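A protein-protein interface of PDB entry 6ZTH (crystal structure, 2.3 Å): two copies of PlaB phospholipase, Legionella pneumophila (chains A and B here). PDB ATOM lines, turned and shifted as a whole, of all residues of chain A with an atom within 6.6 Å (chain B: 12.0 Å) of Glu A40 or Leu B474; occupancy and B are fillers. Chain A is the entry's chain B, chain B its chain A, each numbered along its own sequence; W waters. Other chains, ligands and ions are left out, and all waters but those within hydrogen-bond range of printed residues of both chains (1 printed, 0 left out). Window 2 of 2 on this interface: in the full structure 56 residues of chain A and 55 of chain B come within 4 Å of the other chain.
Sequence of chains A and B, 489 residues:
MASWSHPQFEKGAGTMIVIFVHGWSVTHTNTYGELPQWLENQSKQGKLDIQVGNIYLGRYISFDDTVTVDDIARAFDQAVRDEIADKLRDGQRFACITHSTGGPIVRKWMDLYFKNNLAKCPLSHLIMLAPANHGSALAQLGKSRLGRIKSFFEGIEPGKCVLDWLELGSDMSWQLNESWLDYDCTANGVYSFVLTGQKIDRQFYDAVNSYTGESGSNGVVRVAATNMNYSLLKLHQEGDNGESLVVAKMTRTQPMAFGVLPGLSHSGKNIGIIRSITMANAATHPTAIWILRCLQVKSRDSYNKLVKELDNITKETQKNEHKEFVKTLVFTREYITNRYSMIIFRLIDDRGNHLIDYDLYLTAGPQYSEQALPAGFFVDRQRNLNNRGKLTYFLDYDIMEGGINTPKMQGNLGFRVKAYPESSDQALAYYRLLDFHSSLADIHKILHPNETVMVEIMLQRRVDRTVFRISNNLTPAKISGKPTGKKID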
ATOM      1  N   PHE A  20       8.578  32.989 -10.254  1.00  0.00           N
ATOM      2  CA  PHE A  20       8.397  32.133  -9.091  1.00  0.00           C
ATOM      3  C   PHE A  20       9.416  32.496  -8.020  1.00  0.00           C
ATOM      4  O   PHE A  20      10.569  32.811  -8.323  1.00  0.00           O
ATOM      5  CB  PHE A  20       8.557  30.661  -9.472  1.00  0.00           C
ATOM      6  CG  PHE A  20       7.410  30.108 -10.263  1.00  0.00           C
ATOM      7  CD1 PHE A  20       7.309  30.345 -11.622  1.00  0.00           C
ATOM      8  CD2 PHE A  20       6.435  29.343  -9.647  1.00  0.00           C
ATOM      9  CE1 PHE A  20       6.256  29.832 -12.349  1.00  0.00           C
ATOM     10  CE2 PHE A  20       5.382  28.829 -10.367  1.00  0.00           C
ATOM     11  CZ  PHE A  20       5.291  29.073 -11.720  1.00  0.00           C
ATOM     12  N   THR A  29      15.323  24.029  -7.555  1.00  0.00           N
ATOM     13  CA  THR A  29      14.187  24.732  -8.136  1.00  0.00           C
ATOM     14  C   THR A  29      13.006  23.817  -8.434  1.00  0.00           C
ATOM     15  O   THR A  29      11.936  24.316  -8.801  1.00  0.00           O
ATOM     16  CB  THR A  29      14.606  25.457  -9.418  1.00  0.00           C
ATOM     17  OG1 THR A  29      15.454  24.609 -10.201  1.00  0.00           O
ATOM     18  CG2 THR A  29      15.347  26.744  -9.079  1.00  0.00           C
ATOM     19  N   GLY A  33       7.532  22.283  -7.986  1.00  0.00           N
ATOM     20  CA  GLY A  33       6.826  21.219  -8.676  1.00  0.00           C
ATOM     21  C   GLY A  33       6.947  21.391 -10.174  1.00  0.00           C
ATOM     22  O   GLY A  33       8.004  21.762 -10.699  1.00  0.00           O
ATOM     23  N   LEU A  35       4.447  23.297 -11.736  1.00  0.00           N
ATOM     24  CA  LEU A  35       3.540  24.402 -12.034  1.00  0.00           C
ATOM     25  C   LEU A  35       4.088  25.344 -13.097  1.00  0.00           C
ATOM     26  O   LEU A  35       3.313  25.749 -13.981  1.00  0.00           O
ATOM     27  CB  LEU A  35       3.223  25.168 -10.744  1.00  0.00           C
ATOM     28  CG  LEU A  35       2.179  26.284 -10.831  1.00  0.00           C
ATOM     29  CD1 LEU A  35       0.879  25.781 -11.437  1.00  0.00           C
ATOM     30  CD2 LEU A  35       1.935  26.886  -9.448  1.00  0.00           C
ATOM     31  N   PRO A  36       5.370  25.727 -13.087  1.00  0.00           N
ATOM     32  CA  PRO A  36       5.869  26.611 -14.158  1.00  0.00           C
ATOM     33  C   PRO A  36       5.604  26.067 -15.553  1.00  0.00           C
ATOM     34  O   PRO A  36       5.070  26.785 -16.408  1.00  0.00           O
ATOM     35  CB  PRO A  36       7.372  26.712 -13.853  1.00  0.00           C
ATOM     36  CG  PRO A  36       7.489  26.409 -12.396  1.00  0.00           C
ATOM     37  CD  PRO A  36       6.418  25.400 -12.101  1.00  0.00           C
ATOM     38  N   GLN A  37       5.969  24.806 -15.806  1.00  0.00           N
ATOM     39  CA  GLN A  37       5.687  24.201 -17.103  1.00  0.00           C
ATOM     40  C   GLN A  37       4.197  24.247 -17.417  1.00  0.00           C
ATOM     41  O   GLN A  37       3.803  24.446 -18.573  1.00  0.00           O
ATOM     42  CB  GLN A  37       6.185  22.755 -17.128  1.00  0.00           C
ATOM     43  CG  GLN A  37       7.695  22.607 -17.050  1.00  0.00           C
ATOM     44  CD  GLN A  37       8.161  22.097 -15.700  1.00  0.00           C
ATOM     45  OE1 GLN A  37       7.874  22.699 -14.664  1.00  0.00           O
ATOM     46  NE2 GLN A  37       8.883  20.981 -15.704  1.00  0.00           N
ATOM     47  N   TRP A  38       3.355  24.065 -16.400  1.00  0.00           N
ATOM     48  CA  TRP A  38       1.914  24.052 -16.627  1.00  0.00           C
ATOM     49  C   TRP A  38       1.429  25.399 -17.149  1.00  0.00           C
ATOM     50  O   TRP A  38       0.712  25.466 -18.153  1.00  0.00           O
ATOM     51  CB  TRP A  38       1.184  23.683 -15.336  1.00  0.00           C
ATOM     52  CG  TRP A  38      -0.281  23.450 -15.532  1.00  0.00           C
ATOM     53  CD1 TRP A  38      -0.863  22.399 -16.177  1.00  0.00           C
ATOM     54  CD2 TRP A  38      -1.352  24.290 -15.086  1.00  0.00           C
ATOM     55  NE1 TRP A  38      -2.231  22.529 -16.156  1.00  0.00           N
ATOM     56  CE2 TRP A  38      -2.556  23.683 -15.493  1.00  0.00           C
ATOM     57  CE3 TRP A  38      -1.410  25.495 -14.379  1.00  0.00           C
ATOM     58  CZ2 TRP A  38      -3.804  24.240 -15.218  1.00  0.00           C
ATOM     59  CZ3 TRP A  38      -2.650  26.047 -14.106  1.00  0.00           C
ATOM     60  CH2 TRP A  38      -3.830  25.419 -14.526  1.00  0.00           C
ATOM     61  N   LEU A  39       1.817  26.489 -16.484  1.00  0.00           N
ATOM     62  CA  LEU A  39       1.312  27.801 -16.875  1.00  0.00           C
ATOM     63  C   LEU A  39       1.783  28.170 -18.277  1.00  0.00           C
ATOM     64  O   LEU A  39       0.998  28.655 -19.100  1.00  0.00           O
ATOM     65  CB  LEU A  39       1.742  28.861 -15.861  1.00  0.00           C
ATOM     66  CG  LEU A  39       1.662  28.486 -14.382  1.00  0.00           C
ATOM     67  CD1 LEU A  39       2.713  29.264 -13.613  1.00  0.00           C
ATOM     68  CD2 LEU A  39       0.282  28.744 -13.802  1.00  0.00           C
ATOM     69  N   GLU A  40       3.069  27.952 -18.566  1.00  0.00           N
ATOM     70  CA  GLU A  40       3.545  28.116 -19.937  1.00  0.00           C
ATOM     71  C   GLU A  40       2.728  27.257 -20.891  1.00  0.00           C
ATOM     72  O   GLU A  40       2.346  27.707 -21.978  1.00  0.00           O
ATOM     73  CB  GLU A  40       5.027  27.751 -20.033  1.00  0.00           C
ATOM     74  CG  GLU A  40       5.398  26.994 -21.305  1.00  0.00           C
ATOM     75  CD  GLU A  40       6.896  26.820 -21.472  1.00  0.00           C
ATOM     76  OE1 GLU A  40       7.353  25.662 -21.571  1.00  0.00           O
ATOM     77  OE2 GLU A  40       7.615  27.842 -21.507  1.00  0.00           O
ATOM     78  N   ASN A  41       2.453  26.011 -20.499  1.00  0.00           N
ATOM     79  CA  ASN A  41       1.667  25.125 -21.346  1.00  0.00           C
ATOM     80  C   ASN A  41       0.211  25.567 -21.413  1.00  0.00           C
ATOM     81  O   ASN A  41      -0.449  25.354 -22.435  1.00  0.00           O
ATOM     82  CB  ASN A  41       1.773  23.690 -20.828  1.00  0.00           C
ATOM     83  CG  ASN A  41       0.957  22.713 -21.646  1.00  0.00           C
ATOM     84  OD1 ASN A  41       1.080  22.652 -22.870  1.00  0.00           O
ATOM     85  ND2 ASN A  41       0.118  21.936 -20.972  1.00  0.00           N
ATOM     86  N   GLN A  42      -0.303  26.187 -20.347  1.00  0.00           N
ATOM     87  CA  GLN A  42      -1.666  26.706 -20.383  1.00  0.00           C
ATOM     88  C   GLN A  42      -1.752  27.957 -21.249  1.00  0.00           C
ATOM     89  O   GLN A  42      -2.729  28.145 -21.984  1.00  0.00           O
ATOM     90  CB  GLN A  42      -2.155  27.008 -18.966  1.00  0.00           C
ATOM     91  CG  GLN A  42      -2.355  25.781 -18.091  1.00  0.00           C
ATOM     92  CD  GLN A  42      -3.571  24.970 -18.490  1.00  0.00           C
ATOM     93  OE1 GLN A  42      -4.688  25.483 -18.532  1.00  0.00           O
ATOM     94  NE2 GLN A  42      -3.359  23.692 -18.782  1.00  0.00           N
ATOM     95  N   SER A  43      -0.743  28.827 -21.171  1.00  0.00           N
ATOM     96  CA  SER A  43      -0.726  30.012 -22.021  1.00  0.00           C
ATOM     97  C   SER A  43      -0.714  29.636 -23.495  1.00  0.00           C
ATOM     98  O   SER A  43      -1.300  30.342 -24.324  1.00  0.00           O
ATOM     99  CB  SER A  43       0.488  30.880 -21.688  1.00  0.00           C
ATOM    100  OG  SER A  43       0.795  31.754 -22.759  1.00  0.00           O
ATOM    101  N   LYS A  44      -0.052  28.528 -23.841  1.00  0.00           N
ATOM    102  CA  LYS A  44      -0.035  28.065 -25.222  1.00  0.00           C
ATOM    103  C   LYS A  44      -1.423  27.690 -25.721  1.00  0.00           C
ATOM    104  O   LYS A  44      -1.635  27.629 -26.937  1.00  0.00           O
ATOM    105  CB  LYS A  44       0.909  26.865 -25.351  1.00  0.00           C
ATOM    106  CG  LYS A  44       1.209  26.456 -26.787  1.00  0.00           C
ATOM    107  CD  LYS A  44       2.168  25.267 -26.858  1.00  0.00           C
ATOM    108  CE  LYS A  44       1.632  24.046 -26.119  1.00  0.00           C
ATOM    109  NZ  LYS A  44       1.586  22.835 -26.987  1.00  0.00           N
ATOM    110  N   GLN A  45      -2.369  27.441 -24.817  1.00  0.00           N
ATOM    111  CA  GLN A  45      -3.726  27.061 -25.183  1.00  0.00           C
ATOM    112  C   GLN A  45      -4.717  28.212 -25.055  1.00  0.00           C
ATOM    113  O   GLN A  45      -5.929  27.983 -25.112  1.00  0.00           O
ATOM    114  CB  GLN A  45      -4.189  25.882 -24.326  1.00  0.00           C
ATOM    115  CG  GLN A  45      -3.085  24.890 -24.005  1.00  0.00           C
ATOM    116  CD  GLN A  45      -3.614  23.542 -23.560  1.00  0.00           C
ATOM    117  OE1 GLN A  45      -3.073  22.499 -23.930  1.00  0.00           O
ATOM    118  NE2 GLN A  45      -4.670  23.554 -22.756  1.00  0.00           N
ATOM    119  N   LEU A  48      -3.791  31.904 -20.851  1.00  0.00           N
ATOM    120  CA  LEU A  48      -2.970  32.983 -20.324  1.00  0.00           C
ATOM    121  C   LEU A  48      -2.209  33.615 -21.482  1.00  0.00           C
ATOM    122  O   LEU A  48      -1.962  32.970 -22.505  1.00  0.00           O
ATOM    123  CB  LEU A  48      -1.984  32.496 -19.255  1.00  0.00           C
ATOM    124  CG  LEU A  48      -2.573  32.058 -17.914  1.00  0.00           C
ATOM    125  CD1 LEU A  48      -1.640  31.072 -17.220  1.00  0.00           C
ATOM    126  CD2 LEU A  48      -2.844  33.257 -17.021  1.00  0.00           C
ATOM    127  N   ILE A  50       1.039  34.633 -21.857  1.00  0.00           N
ATOM    128  CA  ILE A  50       2.436  34.569 -21.444  1.00  0.00           C
ATOM    129  C   ILE A  50       3.236  34.040 -22.625  1.00  0.00           C
ATOM    130  O   ILE A  50       3.135  32.856 -22.974  1.00  0.00           O
ATOM    131  CB  ILE A  50       2.633  33.681 -20.207  1.00  0.00           C
ATOM    132  CG1 ILE A  50       1.645  34.064 -19.104  1.00  0.00           C
ATOM    133  CG2 ILE A  50       4.065  33.794 -19.698  1.00  0.00           C
ATOM    134  CD1 ILE A  50       1.607  33.084 -17.948  1.00  0.00           C
ATOM    135  N   GLN A  51       4.032  34.908 -23.241  1.00  0.00           N
ATOM    136  CA  GLN A  51       4.852  34.500 -24.369  1.00  0.00           C
ATOM    137  C   GLN A  51       5.937  33.526 -23.916  1.00  0.00           C
ATOM    138  O   GLN A  51       6.347  33.505 -22.751  1.00  0.00           O
ATOM    139  CB  GLN A  51       5.485  35.718 -25.040  1.00  0.00           C
ATOM    140  CG  GLN A  51       4.477  36.722 -25.582  1.00  0.00           C
ATOM    141  CD  GLN A  51       5.087  38.090 -25.826  1.00  0.00           C
ATOM    142  OE1 GLN A  51       6.299  38.273 -25.704  1.00  0.00           O
ATOM    143  NE2 GLN A  51       4.248  39.060 -26.173  1.00  0.00           N
ATOM    144  N   VAL A  52       6.402  32.705 -24.861  1.00  0.00           N
ATOM    145  CA  VAL A  52       7.446  31.736 -24.553  1.00  0.00           C
ATOM    146  C   VAL A  52       8.661  32.465 -23.998  1.00  0.00           C
ATOM    147  O   VAL A  52       9.136  33.451 -24.575  1.00  0.00           O
ATOM    148  CB  VAL A  52       7.807  30.916 -25.802  1.00  0.00           C
ATOM    149  CG1 VAL A  52       6.653  29.999 -26.186  1.00  0.00           C
ATOM    150  CG2 VAL A  52       8.183  31.828 -26.965  1.00  0.00           C
ATOM    151  N   GLY A  53       9.166  31.983 -22.865  1.00  0.00           N
ATOM    152  CA  GLY A  53      10.309  32.591 -22.221  1.00  0.00           C
ATOM    153  C   GLY A  53       9.990  33.680 -21.226  1.00  0.00           C
ATOM    154  O   GLY A  53      10.917  34.345 -20.745  1.00  0.00           O
ATOM    155  N   ASN A  54       8.715  33.891 -20.901  1.00  0.00           N
ATOM    156  CA  ASN A  54       8.311  34.907 -19.940  1.00  0.00           C
ATOM    157  C   ASN A  54       7.946  34.311 -18.583  1.00  0.00           C
ATOM    158  O   ASN A  54       7.321  34.989 -17.760  1.00  0.00           O
ATOM    159  CB  ASN A  54       7.142  35.722 -20.497  1.00  0.00           C
ATOM    160  CG  ASN A  54       7.604  36.949 -21.266  1.00  0.00           C
ATOM    161  OD1 ASN A  54       8.786  37.090 -21.579  1.00  0.00           O
ATOM    162  ND2 ASN A  54       6.671  37.843 -21.571  1.00  0.00           N
ATOM    163  N   ILE A  55       8.324  33.061 -18.332  1.00  0.00           N
ATOM    164  CA  ILE A  55       8.154  32.418 -17.033  1.00  0.00           C
ATOM    165  C   ILE A  55       9.544  32.180 -16.460  1.00  0.00           C
ATOM    166  O   ILE A  55      10.376  31.513 -17.086  1.00  0.00           O
ATOM    167  CB  ILE A  55       7.361  31.107 -17.145  1.00  0.00           C
ATOM    168  CG1 ILE A  55       6.056  31.355 -17.907  1.00  0.00           C
ATOM    169  CG2 ILE A  55       7.074  30.533 -15.762  1.00  0.00           C
ATOM    170  CD1 ILE A  55       5.028  30.253 -17.757  1.00  0.00           C
ATOM    171  N   TYR A  56       9.796  32.728 -15.273  1.00  0.00           N
ATOM    172  CA  TYR A  56      11.113  32.699 -14.655  1.00  0.00           C
ATOM    173  C   TYR A  56      11.075  31.903 -13.359  1.00  0.00           C
ATOM    174  O   TYR A  56      10.128  32.017 -12.574  1.00  0.00           O
ATOM    175  CB  TYR A  56      11.616  34.119 -14.365  1.00  0.00           C
ATOM    176  CG  TYR A  56      12.069  34.872 -15.593  1.00  0.00           C
ATOM    177  CD1 TYR A  56      11.153  35.306 -16.542  1.00  0.00           C
ATOM    178  CD2 TYR A  56      13.413  35.147 -15.805  1.00  0.00           C
ATOM    179  CE1 TYR A  56      11.563  35.994 -17.667  1.00  0.00           C
ATOM    180  CE2 TYR A  56      13.833  35.833 -16.926  1.00  0.00           C
ATOM    181  CZ  TYR A  56      12.904  36.254 -17.854  1.00  0.00           C
ATOM    182  OH  TYR A  56      13.317  36.938 -18.974  1.00  0.00           O
ATOM    183  N   LEU A  57      12.113  31.103 -13.141  1.00  0.00           N
ATOM    184  CA  LEU A  57      12.307  30.386 -11.889  1.00  0.00           C
ATOM    185  C   LEU A  57      13.244  31.206 -11.012  1.00  0.00           C
ATOM    186  O   LEU A  57      14.393  31.461 -11.389  1.00  0.00           O
ATOM    187  CB  LEU A  57      12.881  28.993 -12.136  1.00  0.00           C
ATOM    188  CG  LEU A  57      12.048  28.050 -13.008  1.00  0.00           C
ATOM    189  CD1 LEU A  57      12.649  26.651 -12.987  1.00  0.00           C
ATOM    190  CD2 LEU A  57      10.596  28.016 -12.561  1.00  0.00           C
ATOM    191  N   ARG B 469      18.771  35.440  -8.010  1.00  0.00           N
ATOM    192  CA  ARG B 469      18.779  35.465  -9.463  1.00  0.00           C
ATOM    193  C   ARG B 469      17.499  34.813  -9.961  1.00  0.00           C
ATOM    194  O   ARG B 469      16.911  33.965  -9.283  1.00  0.00           O
ATOM    195  CB  ARG B 469      19.996  34.736 -10.051  1.00  0.00           C
ATOM    196  CG  ARG B 469      21.342  35.268  -9.578  1.00  0.00           C
ATOM    197  CD  ARG B 469      21.864  36.377 -10.482  1.00  0.00           C
ATOM    198  NE  ARG B 469      21.376  37.692 -10.076  1.00  0.00           N
ATOM    199  CZ  ARG B 469      21.388  38.771 -10.853  1.00  0.00           C
ATOM    200  NH1 ARG B 469      21.866  38.700 -12.088  1.00  0.00           N
ATOM    201  NH2 ARG B 469      20.921  39.923 -10.394  1.00  0.00           N
ATOM    202  N   ILE B 470      17.066  35.220 -11.151  1.00  0.00           N
ATOM    203  CA  ILE B 470      15.906  34.635 -11.809  1.00  0.00           C
ATOM    204  C   ILE B 470      16.320  34.217 -13.212  1.00  0.00           C
ATOM    205  O   ILE B 470      17.069  34.931 -13.889  1.00  0.00           O
ATOM    206  CB  ILE B 470      14.710  35.609 -11.853  1.00  0.00           C
ATOM    207  CG1 ILE B 470      14.997  36.789 -12.780  1.00  0.00           C
ATOM    208  CG2 ILE B 470      14.379  36.098 -10.446  1.00  0.00           C
ATOM    209  CD1 ILE B 470      13.906  37.843 -12.783  1.00  0.00           C
ATOM    210  N   SER B 471      15.841  33.053 -13.642  1.00  0.00           N
ATOM    211  CA  SER B 471      16.173  32.501 -14.946  1.00  0.00           C
ATOM    212  C   SER B 471      14.940  31.840 -15.537  1.00  0.00           C
ATOM    213  O   SER B 471      14.189  31.166 -14.825  1.00  0.00           O
ATOM    214  CB  SER B 471      17.315  31.485 -14.844  1.00  0.00           C
ATOM    215  OG  SER B 471      17.285  30.580 -15.931  1.00  0.00           O
ATOM    216  N   ASN B 472      14.737  32.033 -16.840  1.00  0.00           N
ATOM    217  CA  ASN B 472      13.595  31.465 -17.543  1.00  0.00           C
ATOM    218  C   ASN B 472      13.869  30.057 -18.062  1.00  0.00           C
ATOM    219  O   ASN B 472      13.140  29.573 -18.936  1.00  0.00           O
ATOM    220  CB  ASN B 472      13.172  32.380 -18.694  1.00  0.00           C
ATOM    221  CG  ASN B 472      14.245  32.525 -19.756  1.00  0.00           C
ATOM    222  OD1 ASN B 472      15.298  31.891 -19.687  1.00  0.00           O
ATOM    223  ND2 ASN B 472      13.980  33.366 -20.749  1.00  0.00           N
ATOM    224  N   ASN B 473      14.905  29.396 -17.554  1.00  0.00           N
ATOM    225  CA  ASN B 473      15.152  27.990 -17.860  1.00  0.00           C
ATOM    226  C   ASN B 473      14.293  27.159 -16.915  1.00  0.00           C
ATOM    227  O   ASN B 473      14.639  26.964 -15.748  1.00  0.00           O
ATOM    228  CB  ASN B 473      16.631  27.655 -17.715  1.00  0.00           C
ATOM    229  CG  ASN B 473      16.960  26.257 -18.198  1.00  0.00           C
ATOM    230  OD1 ASN B 473      16.100  25.377 -18.217  1.00  0.00           O
ATOM    231  ND2 ASN B 473      18.209  26.046 -18.594  1.00  0.00           N
ATOM    232  N   LEU B 474      13.159  26.670 -17.419  1.00  0.00           N
ATOM    233  CA  LEU B 474      12.209  25.948 -16.582  1.00  0.00           C
ATOM    234  C   LEU B 474      12.685  24.553 -16.195  1.00  0.00           C
ATOM    235  O   LEU B 474      11.954  23.854 -15.484  1.00  0.00           O
ATOM    236  CB  LEU B 474      10.860  25.850 -17.297  1.00  0.00           C
ATOM    237  CG  LEU B 474      10.259  27.174 -17.771  1.00  0.00           C
ATOM    238  CD1 LEU B 474       8.842  26.962 -18.286  1.00  0.00           C
ATOM    239  CD2 LEU B 474      10.276  28.216 -16.660  1.00  0.00           C
ATOM    240  N   THR B 475      13.869  24.129 -16.636  1.00  0.00           N
ATOM    241  CA  THR B 475      14.413  22.835 -16.227  1.00  0.00           C
ATOM    242  C   THR B 475      14.929  22.957 -14.797  1.00  0.00           C
ATOM    243  O   THR B 475      15.887  23.702 -14.549  1.00  0.00           O
ATOM    244  CB  THR B 475      15.529  22.382 -17.166  1.00  0.00           C
ATOM    245  OG1 THR B 475      14.965  21.930 -18.409  1.00  0.00           O
ATOM    246  CG2 THR B 475      16.328  21.244 -16.542  1.00  0.00           C
ATOM    247  N   PRO B 476      14.330  22.257 -13.829  1.00  0.00           N
ATOM    248  CA  PRO B 476      14.793  22.392 -12.441  1.00  0.00           C
ATOM    249  C   PRO B 476      16.281  22.105 -12.313  1.00  0.00           C
ATOM    250  O   PRO B 476      16.850  21.299 -13.053  1.00  0.00           O
ATOM    251  CB  PRO B 476      13.954  21.358 -11.679  1.00  0.00           C
ATOM    252  CG  PRO B 476      12.749  21.136 -12.526  1.00  0.00           C
ATOM    253  CD  PRO B 476      13.198  21.318 -13.949  1.00  0.00           C
ATOM    254  N   ALA B 477      16.910  22.782 -11.356  1.00  0.00           N
ATOM    255  CA  ALA B 477      18.343  22.652 -11.141  1.00  0.00           C
ATOM    256  C   ALA B 477      18.657  23.027  -9.701  1.00  0.00           C
ATOM    257  O   ALA B 477      17.890  23.733  -9.043  1.00  0.00           O
ATOM    258  CB  ALA B 477      19.138  23.533 -12.111  1.00  0.00           C
ATOM    259  N   LYS B 478      19.799  22.539  -9.221  1.00  0.00           N
ATOM    260  CA  LYS B 478      20.250  22.877  -7.879  1.00  0.00           C
ATOM    261  C   LYS B 478      20.620  24.355  -7.806  1.00  0.00           C
ATOM    262  O   LYS B 478      21.028  24.970  -8.797  1.00  0.00           O
ATOM    263  CB  LYS B 478      21.449  22.018  -7.479  1.00  0.00           C
ATOM    264  CG  LYS B 478      21.091  20.644  -6.913  1.00  0.00           C
ATOM    265  CD  LYS B 478      20.314  20.744  -5.605  1.00  0.00           C
ATOM    266  CE  LYS B 478      20.059  19.368  -5.003  1.00  0.00           C
ATOM    267  NZ  LYS B 478      19.550  19.455  -3.604  1.00  0.00           N
ATOM    268  N   ILE B 479      20.480  24.924  -6.613  1.00  0.00           N
ATOM    269  CA  ILE B 479      20.701  26.346  -6.382  1.00  0.00           C
ATOM    270  C   ILE B 479      22.113  26.520  -5.842  1.00  0.00           C
ATOM    271  O   ILE B 479      22.417  26.105  -4.718  1.00  0.00           O
ATOM    272  CB  ILE B 479      19.658  26.927  -5.418  1.00  0.00           C
ATOM    273  CG1 ILE B 479      18.274  26.887  -6.066  1.00  0.00           C
ATOM    274  CG2 ILE B 479      20.032  28.348  -5.027  1.00  0.00           C
ATOM    275  CD1 ILE B 479      17.140  26.760  -5.078  1.00  0.00           C
HETATM  276  O   HOH W   1      10.070  24.284 -13.283  1.00  0.00           O
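Water W1 lies within hydrogen-bond range of O of Leu B474 and OE1 of Gln A37.
OG of Ser B471 lies within hydrogen-bond range of N of Asn B473, at 3.1 Å.
The side-chain amide oxygen (OD1) of Asn B473 lies within hydrogen-bond range of the backbone NH (N) of Thr B475.
N of Phe A20 is in hydrogen-bond range of O of Tyr A56, at 3.0 Å.
Thr A29 touches Pro B476 (OG1 to CA, 3.2 Å).
OE2 of Glu A40 touches CD1 of Leu B474 (3.6 Å).
Asn B472 touches Ile A55.
Ile A55 touches Leu B474 (O to CD2, 3.3 Å).
CG1 of Ile B470 touches CD2 of Tyr A56 (3.8 Å).
Ser B471 touches Tyr A56 (O to CA, 3.4 Å).
Tyr A56 touches Asn B472 (CD2 to N, 3.5 Å).
Ile B470 touches Leu A57.
Leu A57 touches Asn B473.
CD1 of Leu A57 touches CA of Leu B474 (3.7 Å).
Of the printed residues of chain B, Thr A29 touches Pro B476 and Ala B477.
Pro A36 touches none of the printed residues of chain B.
No residue of chain B comes within 4 Å of Gln A37.
No residue of chain B comes within 4 Å of Leu A39.
Glu A40 touches one residue of chain B.
No residue of chain B comes within 4 Å of Asn A41.
Leu A48 touches none of the printed residues of chain B.
Ile A50 touches none of the printed residues of chain B.
No residue of chain B comes within 4 Å of Val A52.
Ile A55 touches two residues of chain B.
Leu A57 touches four residues of chain B.
Printed residues of chain A within 4 Å of Ser B471: Tyr A56 (3.4 Å) and Leu A57 (2.7 Å).
Of chain A, only Glu A40, Ile A55 and Leu A57 come within 4 Å of Leu B474.
Of the printed residues of chain A, Pro B476 touches Thr A29 (3.2 Å).
The nearest residue of chain B that does not touch Glu A40 is Asn B472 (6.3 Å).
The nearest residue of chain A that does not touch Leu B474 is Gln A37 (4.2 Å).
No position is printed for both chains.
Of the 13 pairs that touch across the chains among the printed residues, none has its exchanged pair printed and touching as well.
Of the 23 printed residues of chain A, 6 touch a printed residue of chain B.
Hydrophobic or aromatic side chains of chain B within 4 Å of the printed part of chain A: Ile B470, Leu B474 and Pro B476.
Among the printed residues, no Asp or Glu carboxylate lies within 4 Å of a Lys or Arg side-chain nitrogen of the other chain.
The side-chain amide nitrogen of Asn B472 lies within hydrogen-bond range of the backbone carbonyl oxygen of Gly A53, at 3.2 Å.
OG1 of Thr A29 sits at hydrogen-bond distance from N of Ala B477, 2.6 Å away.
O of Ser B471 lies within hydrogen-bond range of N of Leu A57 (2.7 Å).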
